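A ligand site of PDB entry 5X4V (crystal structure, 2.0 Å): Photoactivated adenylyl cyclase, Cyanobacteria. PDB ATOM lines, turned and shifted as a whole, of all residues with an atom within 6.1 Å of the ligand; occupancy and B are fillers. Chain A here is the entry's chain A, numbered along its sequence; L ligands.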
ATOM      1  N   TYR A   6      10.547   6.058  10.214  1.00  0.00           N
ATOM      2  CA  TYR A   6      10.784   6.141  11.640  1.00  0.00           C
ATOM      3  C   TYR A   6      11.945   5.257  12.136  1.00  0.00           C
ATOM      4  O   TYR A   6      12.446   4.386  11.422  1.00  0.00           O
ATOM      5  CB  TYR A   6       9.496   5.791  12.401  1.00  0.00           C
ATOM      6  CG  TYR A   6       9.261   4.307  12.525  1.00  0.00           C
ATOM      7  CD1 TYR A   6       9.803   3.578  13.584  1.00  0.00           C
ATOM      8  CD2 TYR A   6       8.507   3.617  11.584  1.00  0.00           C
ATOM      9  CE1 TYR A   6       9.609   2.232  13.704  1.00  0.00           C
ATOM     10  CE2 TYR A   6       8.302   2.275  11.696  1.00  0.00           C
ATOM     11  CZ  TYR A   6       8.854   1.579  12.753  1.00  0.00           C
ATOM     12  OH  TYR A   6       8.652   0.223  12.867  1.00  0.00           O
ATOM     13  N   SER A   8      13.249   3.227  15.975  1.00  0.00           N
ATOM     14  CA  SER A   8      12.849   2.916  17.348  1.00  0.00           C
ATOM     15  C   SER A   8      13.869   2.011  18.033  1.00  0.00           C
ATOM     16  O   SER A   8      14.782   1.513  17.397  1.00  0.00           O
ATOM     17  CB  SER A   8      11.454   2.273  17.387  1.00  0.00           C
ATOM     18  OG  SER A   8      11.472   0.988  16.778  1.00  0.00           O
ATOM     19  N   LEU A  14      15.938  -9.123  20.956  1.00  0.00           N
ATOM     20  CA  LEU A  14      15.266  -9.853  19.906  1.00  0.00           C
ATOM     21  C   LEU A  14      16.331 -10.556  19.062  1.00  0.00           C
ATOM     22  O   LEU A  14      17.380  -9.977  18.798  1.00  0.00           O
ATOM     23  CB  LEU A  14      14.414  -8.913  19.040  1.00  0.00           C
ATOM     24  CG  LEU A  14      13.138  -8.325  19.634  1.00  0.00           C
ATOM     25  CD1 LEU A  14      12.469  -7.378  18.662  1.00  0.00           C
ATOM     26  CD2 LEU A  14      12.150  -9.412  20.034  1.00  0.00           C
ATOM     27  N   ILE A  22       8.975 -10.925  12.248  1.00  0.00           N
ATOM     28  CA  ILE A  22       8.213  -9.692  12.195  1.00  0.00           C
ATOM     29  C   ILE A  22       8.253  -9.134  10.771  1.00  0.00           C
ATOM     30  O   ILE A  22       7.311  -8.481  10.326  1.00  0.00           O
ATOM     31  CB  ILE A  22       8.755  -8.645  13.179  1.00  0.00           C
ATOM     32  CG1 ILE A  22       8.465  -9.085  14.625  1.00  0.00           C
ATOM     33  CG2 ILE A  22       8.151  -7.269  12.876  1.00  0.00           C
ATOM     34  CD1 ILE A  22       9.433  -8.549  15.651  1.00  0.00           C
ATOM     35  N   ILE A  25       5.557 -11.541   8.574  1.00  0.00           N
ATOM     36  CA  ILE A  25       4.192 -11.124   8.928  1.00  0.00           C
ATOM     37  C   ILE A  25       3.923  -9.688   8.506  1.00  0.00           C
ATOM     38  O   ILE A  25       2.780  -9.323   8.222  1.00  0.00           O
ATOM     39  CB  ILE A  25       3.931 -11.240  10.436  1.00  0.00           C
ATOM     40  CG1 ILE A  25       4.290 -12.642  10.955  1.00  0.00           C
ATOM     41  CG2 ILE A  25       2.474 -10.888  10.746  1.00  0.00           C
ATOM     42  CD1 ILE A  25       4.061 -12.823  12.459  1.00  0.00           C
ATOM     43  N   SER A  26       4.980  -8.886   8.499  1.00  0.00           N
ATOM     44  CA  SER A  26       4.920  -7.503   8.023  1.00  0.00           C
ATOM     45  C   SER A  26       4.625  -7.462   6.536  1.00  0.00           C
ATOM     46  O   SER A  26       3.734  -6.739   6.095  1.00  0.00           O
ATOM     47  CB  SER A  26       6.234  -6.768   8.310  1.00  0.00           C
ATOM     48  OG  SER A  26       6.031  -5.672   9.179  1.00  0.00           O
ATOM     49  N   LYS A  29       0.818  -8.671   5.592  1.00  0.00           N
ATOM     50  CA  LYS A  29      -0.265  -7.756   5.942  1.00  0.00           C
ATOM     51  C   LYS A  29      -0.144  -6.481   5.123  1.00  0.00           C
ATOM     52  O   LYS A  29      -1.102  -5.725   4.922  1.00  0.00           O
ATOM     53  CB  LYS A  29      -0.257  -7.460   7.433  1.00  0.00           C
ATOM     54  CG  LYS A  29      -1.587  -6.992   7.984  1.00  0.00           C
ATOM     55  CD  LYS A  29      -1.657  -7.212   9.492  1.00  0.00           C
ATOM     56  CE  LYS A  29      -2.941  -6.628  10.072  1.00  0.00           C
ATOM     57  NZ  LYS A  29      -3.124  -6.974  11.518  1.00  0.00           N
ATOM     58  N   ASN A  30       1.080  -6.272   4.635  1.00  0.00           N
ATOM     59  CA  ASN A  30       1.411  -5.179   3.739  1.00  0.00           C
ATOM     60  C   ASN A  30       0.980  -5.444   2.300  1.00  0.00           C
ATOM     61  O   ASN A  30       0.352  -4.589   1.669  1.00  0.00           O
ATOM     62  CB  ASN A  30       2.925  -4.927   3.801  1.00  0.00           C
ATOM     63  CG  ASN A  30       3.309  -4.001   4.926  1.00  0.00           C
ATOM     64  OD1 ASN A  30       2.454  -3.502   5.654  1.00  0.00           O
ATOM     65  ND2 ASN A  30       4.610  -3.753   5.062  1.00  0.00           N
ATOM     66  N   VAL A  35       1.012  -1.747   0.453  1.00  0.00           N
ATOM     67  CA  VAL A  35       2.005  -0.975   1.171  1.00  0.00           C
ATOM     68  C   VAL A  35       3.371  -1.582   0.951  1.00  0.00           C
ATOM     69  O   VAL A  35       3.527  -2.814   0.927  1.00  0.00           O
ATOM     70  CB  VAL A  35       1.695  -0.873   2.688  1.00  0.00           C
ATOM     71  CG1 VAL A  35       0.713   0.266   2.960  1.00  0.00           C
ATOM     72  CG2 VAL A  35       1.153  -2.188   3.188  1.00  0.00           C
ATOM     73  N   LEU A  39      12.697  -2.491   6.291  1.00  0.00           N
ATOM     74  CA  LEU A  39      12.904  -2.610   7.735  1.00  0.00           C
ATOM     75  C   LEU A  39      14.337  -3.048   7.961  1.00  0.00           C
ATOM     76  O   LEU A  39      14.758  -4.106   7.487  1.00  0.00           O
ATOM     77  CB  LEU A  39      11.905  -3.605   8.346  1.00  0.00           C
ATOM     78  CG  LEU A  39      11.864  -3.749   9.855  1.00  0.00           C
ATOM     79  CD1 LEU A  39      12.967  -4.650  10.363  1.00  0.00           C
ATOM     80  CD2 LEU A  39      11.997  -2.378  10.476  1.00  0.00           C
ATOM     81  N   PHE A  46      15.691  -0.237  15.433  1.00  0.00           N
ATOM     82  CA  PHE A  46      14.884  -0.419  14.214  1.00  0.00           C
ATOM     83  C   PHE A  46      14.769   0.844  13.353  1.00  0.00           C
ATOM     84  O   PHE A  46      14.454   1.925  13.863  1.00  0.00           O
ATOM     85  CB  PHE A  46      13.467  -0.886  14.568  1.00  0.00           C
ATOM     86  CG  PHE A  46      13.371  -2.363  14.811  1.00  0.00           C
ATOM     87  CD1 PHE A  46      13.955  -3.266  13.929  1.00  0.00           C
ATOM     88  CD2 PHE A  46      12.706  -2.852  15.921  1.00  0.00           C
ATOM     89  CE1 PHE A  46      13.867  -4.633  14.140  1.00  0.00           C
ATOM     90  CE2 PHE A  46      12.619  -4.219  16.132  1.00  0.00           C
ATOM     91  CZ  PHE A  46      13.208  -5.106  15.249  1.00  0.00           C
ATOM     92  N   PHE A  47      15.034   0.681  12.052  1.00  0.00           N
ATOM     93  CA  PHE A  47      14.727   1.690  11.022  1.00  0.00           C
ATOM     94  C   PHE A  47      13.623   1.169  10.096  1.00  0.00           C
ATOM     95  O   PHE A  47      13.698   0.039   9.620  1.00  0.00           O
ATOM     96  CB  PHE A  47      15.973   2.023  10.180  1.00  0.00           C
ATOM     97  CG  PHE A  47      17.211   2.213  10.994  1.00  0.00           C
ATOM     98  CD1 PHE A  47      17.900   1.123  11.512  1.00  0.00           C
ATOM     99  CD2 PHE A  47      17.712   3.487  11.245  1.00  0.00           C
ATOM    100  CE1 PHE A  47      19.057   1.286  12.257  1.00  0.00           C
ATOM    101  CE2 PHE A  47      18.854   3.661  12.002  1.00  0.00           C
ATOM    102  CZ  PHE A  47      19.538   2.555  12.520  1.00  0.00           C
ATOM    103  N   GLN A  48      12.622   1.975   9.815  1.00  0.00           N
ATOM    104  CA  GLN A  48      11.613   1.559   8.838  1.00  0.00           C
ATOM    105  C   GLN A  48      11.096   2.701   7.960  1.00  0.00           C
ATOM    106  O   GLN A  48      10.845   3.820   8.436  1.00  0.00           O
ATOM    107  CB  GLN A  48      10.423   0.912   9.546  1.00  0.00           C
ATOM    108  CG  GLN A  48       9.397   0.386   8.564  1.00  0.00           C
ATOM    109  CD  GLN A  48       8.451  -0.635   9.146  1.00  0.00           C
ATOM    110  OE1 GLN A  48       7.628  -0.330  10.025  1.00  0.00           O
ATOM    111  NE2 GLN A  48       8.538  -1.866   8.667  1.00  0.00           N
ATOM    112  N   LEU A  50       7.823   3.196   5.406  1.00  0.00           N
ATOM    113  CA  LEU A  50       6.554   2.655   4.889  1.00  0.00           C
ATOM    114  C   LEU A  50       5.850   3.613   3.920  1.00  0.00           C
ATOM    115  O   LEU A  50       5.709   4.816   4.198  1.00  0.00           O
ATOM    116  CB  LEU A  50       5.585   2.321   6.034  1.00  0.00           C
ATOM    117  CG  LEU A  50       6.052   1.505   7.231  1.00  0.00           C
ATOM    118  CD1 LEU A  50       6.011   2.387   8.478  1.00  0.00           C
ATOM    119  CD2 LEU A  50       5.195   0.280   7.414  1.00  0.00           C
ATOM    120  N   ILE A  60      -1.587   1.511  10.102  1.00  0.00           N
ATOM    121  CA  ILE A  60      -0.437   0.664  10.401  1.00  0.00           C
ATOM    122  C   ILE A  60       0.424   1.288  11.501  1.00  0.00           C
ATOM    123  O   ILE A  60       0.837   0.617  12.449  1.00  0.00           O
ATOM    124  CB  ILE A  60       0.442   0.443   9.169  1.00  0.00           C
ATOM    125  CG1 ILE A  60      -0.272  -0.419   8.129  1.00  0.00           C
ATOM    126  CG2 ILE A  60       1.776  -0.176   9.569  1.00  0.00           C
ATOM    127  CD1 ILE A  60       0.612  -0.800   6.978  1.00  0.00           C
ATOM    128  N   ARG A  63      -0.763   1.172  14.994  1.00  0.00           N
ATOM    129  CA  ARG A  63      -0.520  -0.167  15.532  1.00  0.00           C
ATOM    130  C   ARG A  63       0.956  -0.396  15.833  1.00  0.00           C
ATOM    131  O   ARG A  63       1.294  -1.092  16.777  1.00  0.00           O
ATOM    132  CB  ARG A  63      -0.990  -1.243  14.551  1.00  0.00           C
ATOM    133  CG  ARG A  63      -2.493  -1.226  14.248  1.00  0.00           C
ATOM    134  CD  ARG A  63      -2.934  -2.553  13.616  1.00  0.00           C
ATOM    135  NE  ARG A  63      -2.034  -2.999  12.552  1.00  0.00           N
ATOM    136  CZ  ARG A  63      -2.348  -3.000  11.253  1.00  0.00           C
ATOM    137  NH1 ARG A  63      -1.465  -3.422  10.363  1.00  0.00           N
ATOM    138  NH2 ARG A  63      -3.535  -2.573  10.858  1.00  0.00           N
ATOM    139  N   ILE A  64       1.833   0.167  15.006  1.00  0.00           N
ATOM    140  CA  ILE A  64       3.250   0.092  15.307  1.00  0.00           C
ATOM    141  C   ILE A  64       3.562   0.882  16.596  1.00  0.00           C
ATOM    142  O   ILE A  64       4.380   0.453  17.400  1.00  0.00           O
ATOM    143  CB  ILE A  64       4.103   0.626  14.145  1.00  0.00           C
ATOM    144  CG1 ILE A  64       3.748  -0.132  12.863  1.00  0.00           C
ATOM    145  CG2 ILE A  64       5.585   0.507  14.464  1.00  0.00           C
ATOM    146  CD1 ILE A  64       4.554   0.298  11.643  1.00  0.00           C
ATOM    147  N   ASP A  67       2.657  -1.124  19.760  1.00  0.00           N
ATOM    148  CA  ASP A  67       3.329  -2.414  19.875  1.00  0.00           C
ATOM    149  C   ASP A  67       4.480  -2.316  20.876  1.00  0.00           C
ATOM    150  O   ASP A  67       5.327  -1.429  20.770  1.00  0.00           O
ATOM    151  CB  ASP A  67       3.835  -2.854  18.496  1.00  0.00           C
ATOM    152  CG  ASP A  67       4.444  -4.223  18.499  1.00  0.00           C
ATOM    153  OD1 ASP A  67       4.949  -4.674  19.548  1.00  0.00           O
ATOM    154  OD2 ASP A  67       4.419  -4.866  17.421  1.00  0.00           O
ATOM    155  N   ARG A  69       7.122  -4.200  21.532  1.00  0.00           N
ATOM    156  CA  ARG A  69       8.408  -4.846  21.273  1.00  0.00           C
ATOM    157  C   ARG A  69       9.491  -3.829  20.903  1.00  0.00           C
ATOM    158  O   ARG A  69      10.669  -4.190  20.740  1.00  0.00           O
ATOM    159  CB  ARG A  69       8.264  -5.901  20.183  1.00  0.00           C
ATOM    160  CG  ARG A  69       7.503  -7.118  20.645  1.00  0.00           C
ATOM    161  CD  ARG A  69       7.075  -7.965  19.487  1.00  0.00           C
ATOM    162  NE  ARG A  69       5.965  -7.358  18.745  1.00  0.00           N
ATOM    163  CZ  ARG A  69       5.534  -7.798  17.566  1.00  0.00           C
ATOM    164  NH1 ARG A  69       6.132  -8.835  16.999  1.00  0.00           N
ATOM    165  NH2 ARG A  69       4.529  -7.184  16.962  1.00  0.00           N
ATOM    166  N   HIS A  70       9.091  -2.562  20.758  1.00  0.00           N
ATOM    167  CA  HIS A  70      10.053  -1.471  20.619  1.00  0.00           C
ATOM    168  C   HIS A  70       9.570  -0.243  21.399  1.00  0.00           C
ATOM    169  O   HIS A  70       8.426  -0.202  21.833  1.00  0.00           O
ATOM    170  CB  HIS A  70      10.310  -1.122  19.137  1.00  0.00           C
ATOM    171  CG  HIS A  70       9.103  -0.668  18.374  1.00  0.00           C
ATOM    172  ND1 HIS A  70       9.165  -0.292  17.049  1.00  0.00           N
ATOM    173  CD2 HIS A  70       7.794  -0.555  18.728  1.00  0.00           C
ATOM    174  CE1 HIS A  70       7.964   0.051  16.619  1.00  0.00           C
ATOM    175  NE2 HIS A  70       7.115  -0.107  17.621  1.00  0.00           N
ATOM    176  N   SER A  91       7.025  -5.399  -0.401  1.00  0.00           N
ATOM    177  CA  SER A  91       5.930  -5.137   0.521  1.00  0.00           C
ATOM    178  C   SER A  91       6.465  -4.865   1.934  1.00  0.00           C
ATOM    179  O   SER A  91       5.868  -4.095   2.692  1.00  0.00           O
ATOM    180  CB  SER A  91       4.967  -6.329   0.520  1.00  0.00           C
ATOM    181  OG  SER A  91       3.737  -5.985   1.136  1.00  0.00           O
ATOM    182  N   MET A  92       7.578  -5.508   2.280  1.00  0.00           N
ATOM    183  CA  MET A  92       8.324  -5.203   3.501  1.00  0.00           C
ATOM    184  C   MET A  92       9.627  -5.999   3.594  1.00  0.00           C
ATOM    185  O   MET A  92       9.756  -6.878   4.439  1.00  0.00           O
ATOM    186  CB  MET A  92       7.471  -5.488   4.737  1.00  0.00           C
ATOM    187  CG  MET A  92       8.057  -4.961   6.043  1.00  0.00           C
ATOM    188  SD  MET A  92       8.640  -3.237   5.998  1.00  0.00           S
ATOM    189  CE  MET A  92       7.247  -2.373   5.275  1.00  0.00           C
HETATM  190  O1  LIG L   1       5.031  -2.589   8.200  1.00  0.00           O
HETATM  191  C1  LIG L   1       4.286  -3.018   9.104  1.00  0.00           C
HETATM  192  N1  LIG L   1       2.984  -3.243   8.859  1.00  0.00           N
HETATM  193  C2  LIG L   1       2.171  -3.702   9.816  1.00  0.00           C
HETATM  194  O2  LIG L   1       0.961  -3.916   9.550  1.00  0.00           O
HETATM  195  C3  LIG L   1       4.842  -3.288  10.446  1.00  0.00           C
HETATM  196  C4  LIG L   1       3.914  -3.795  11.477  1.00  0.00           C
HETATM  197  N2  LIG L   1       2.636  -3.967  11.064  1.00  0.00           N
HETATM  198  N3  LIG L   1       6.145  -3.068  10.699  1.00  0.00           N
HETATM  199  C5  LIG L   1       6.657  -3.308  11.919  1.00  0.00           C
HETATM  200  C6  LIG L   1       8.007  -3.064  12.132  1.00  0.00           C
HETATM  201  C7  LIG L   1       8.596  -3.285  13.364  1.00  0.00           C
HETATM  202  C8  LIG L   1      10.067  -2.967  13.458  1.00  0.00           C
HETATM  203  C9  LIG L   1       7.713  -3.813  14.473  1.00  0.00           C
HETATM  204  N4  LIG L   1       8.069  -4.147  15.803  1.00  0.00           N
HETATM  205  C10 LIG L   1       9.159  -5.129  15.896  1.00  0.00           C
HETATM  206  C11 LIG L   1       8.329  -2.978  16.627  1.00  0.00           C
HETATM  207  C12 LIG L   1       6.362  -4.052  14.238  1.00  0.00           C
HETATM  208  C13 LIG L   1       5.783  -3.828  13.006  1.00  0.00           C
HETATM  209  N5  LIG L   1       4.416  -4.085  12.787  1.00  0.00           N
HETATM  210  C14 LIG L   1       3.626  -4.586  13.937  1.00  0.00           C
HETATM  211  C15 LIG L   1       2.174  -4.885  13.600  1.00  0.00           C
HETATM  212  O3  LIG L   1       1.466  -3.644  13.658  1.00  0.00           O
HETATM  213  C16 LIG L   1       1.406  -5.862  14.486  1.00  0.00           C
HETATM  214  O4  LIG L   1       2.233  -7.004  14.736  1.00  0.00           O
HETATM  215  C17 LIG L   1       0.100  -6.284  13.775  1.00  0.00           C
HETATM  216  O5  LIG L   1      -0.089  -5.603  12.525  1.00  0.00           O
HETATM  217  C18 LIG L   1      -1.167  -6.059  14.600  1.00  0.00           C
HETATM  218  O6  LIG L   1      -2.233  -6.828  14.025  1.00  0.00           O
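NH1 of Arg 63 is in hydrogen-bond range of O2 of the ligand (2.6 Å).
The side-chain amino group (NZ) of Lys 29 is in hydrogen-bond range of an oxygen (O6) of the ligand.
The side-chain hydroxyl (OG) of Ser 26 lies close to a nitrogen (N3) of the ligand, 3.0 Å away.
The side-chain amide oxygen (OE1) of Gln 48 sits close to a nitrogen (N3) of the ligand, 3.2 Å away.
An oxygen (O4) of the ligand is in hydrogen-bond range of the guanidinium group of Arg 69.
A nitrogen (N1) of the ligand sits at hydrogen-bond distance from the side-chain amide oxygen (OD1) of Asn 30 (3.3 Å).
Tyr 6 touches the ligand.
CD1 of Ile 22 touches C10 of the ligand (3.4 Å).
CD2 of Leu 39 touches C8 of the ligand, at 3.6 Å.
Phe 46 touches the ligand.
Leu 50 touches the ligand (CD2 to O1, 3.0 Å).
Ile 60 touches the ligand (CG2 to N1, 3.4 Å).
Ile 64 touches the ligand.
OD2 of Asp 67 touches C14 of the ligand, 3.6 Å away.
His 70 touches the ligand.
Met 92 touches the ligand (CE to O1, 3.7 Å).
A ring nitrogen (NE2) of His 70 lies within hydrogen-bond range of the backbone carbonyl oxygen (O) of Ile 64 (2.8 Å).
The side-chain hydroxyl (OG) of Ser 8 is in hydrogen-bond range of a ring nitrogen (ND1) of His 70, 2.7 Å away.
The side-chain hydroxyl (OG) of Ser 26 sits close to the backbone carbonyl oxygen (O) of Ile 22, 3.3 Å away.
O of Gln 48 is in hydrogen-bond range of N of Tyr 6, at 2.9 Å.
The side-chain sulfur (SD) of Met 92 sits at hydrogen-bond distance from the side-chain amide nitrogen (NE2) of Gln 48 (3.0 Å).
The guanidinium group (NE) of Arg 69 lies within salt-bridge range of the side-chain carboxylate (OD1) of Asp 67 (3.0 Å).
O of Asn 30 lies close to N of Val 35, at 3.2 Å.
The backbone carbonyl oxygen of Phe 46 sits at hydrogen-bond distance from the backbone NH of Ser 8 (2.8 Å).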
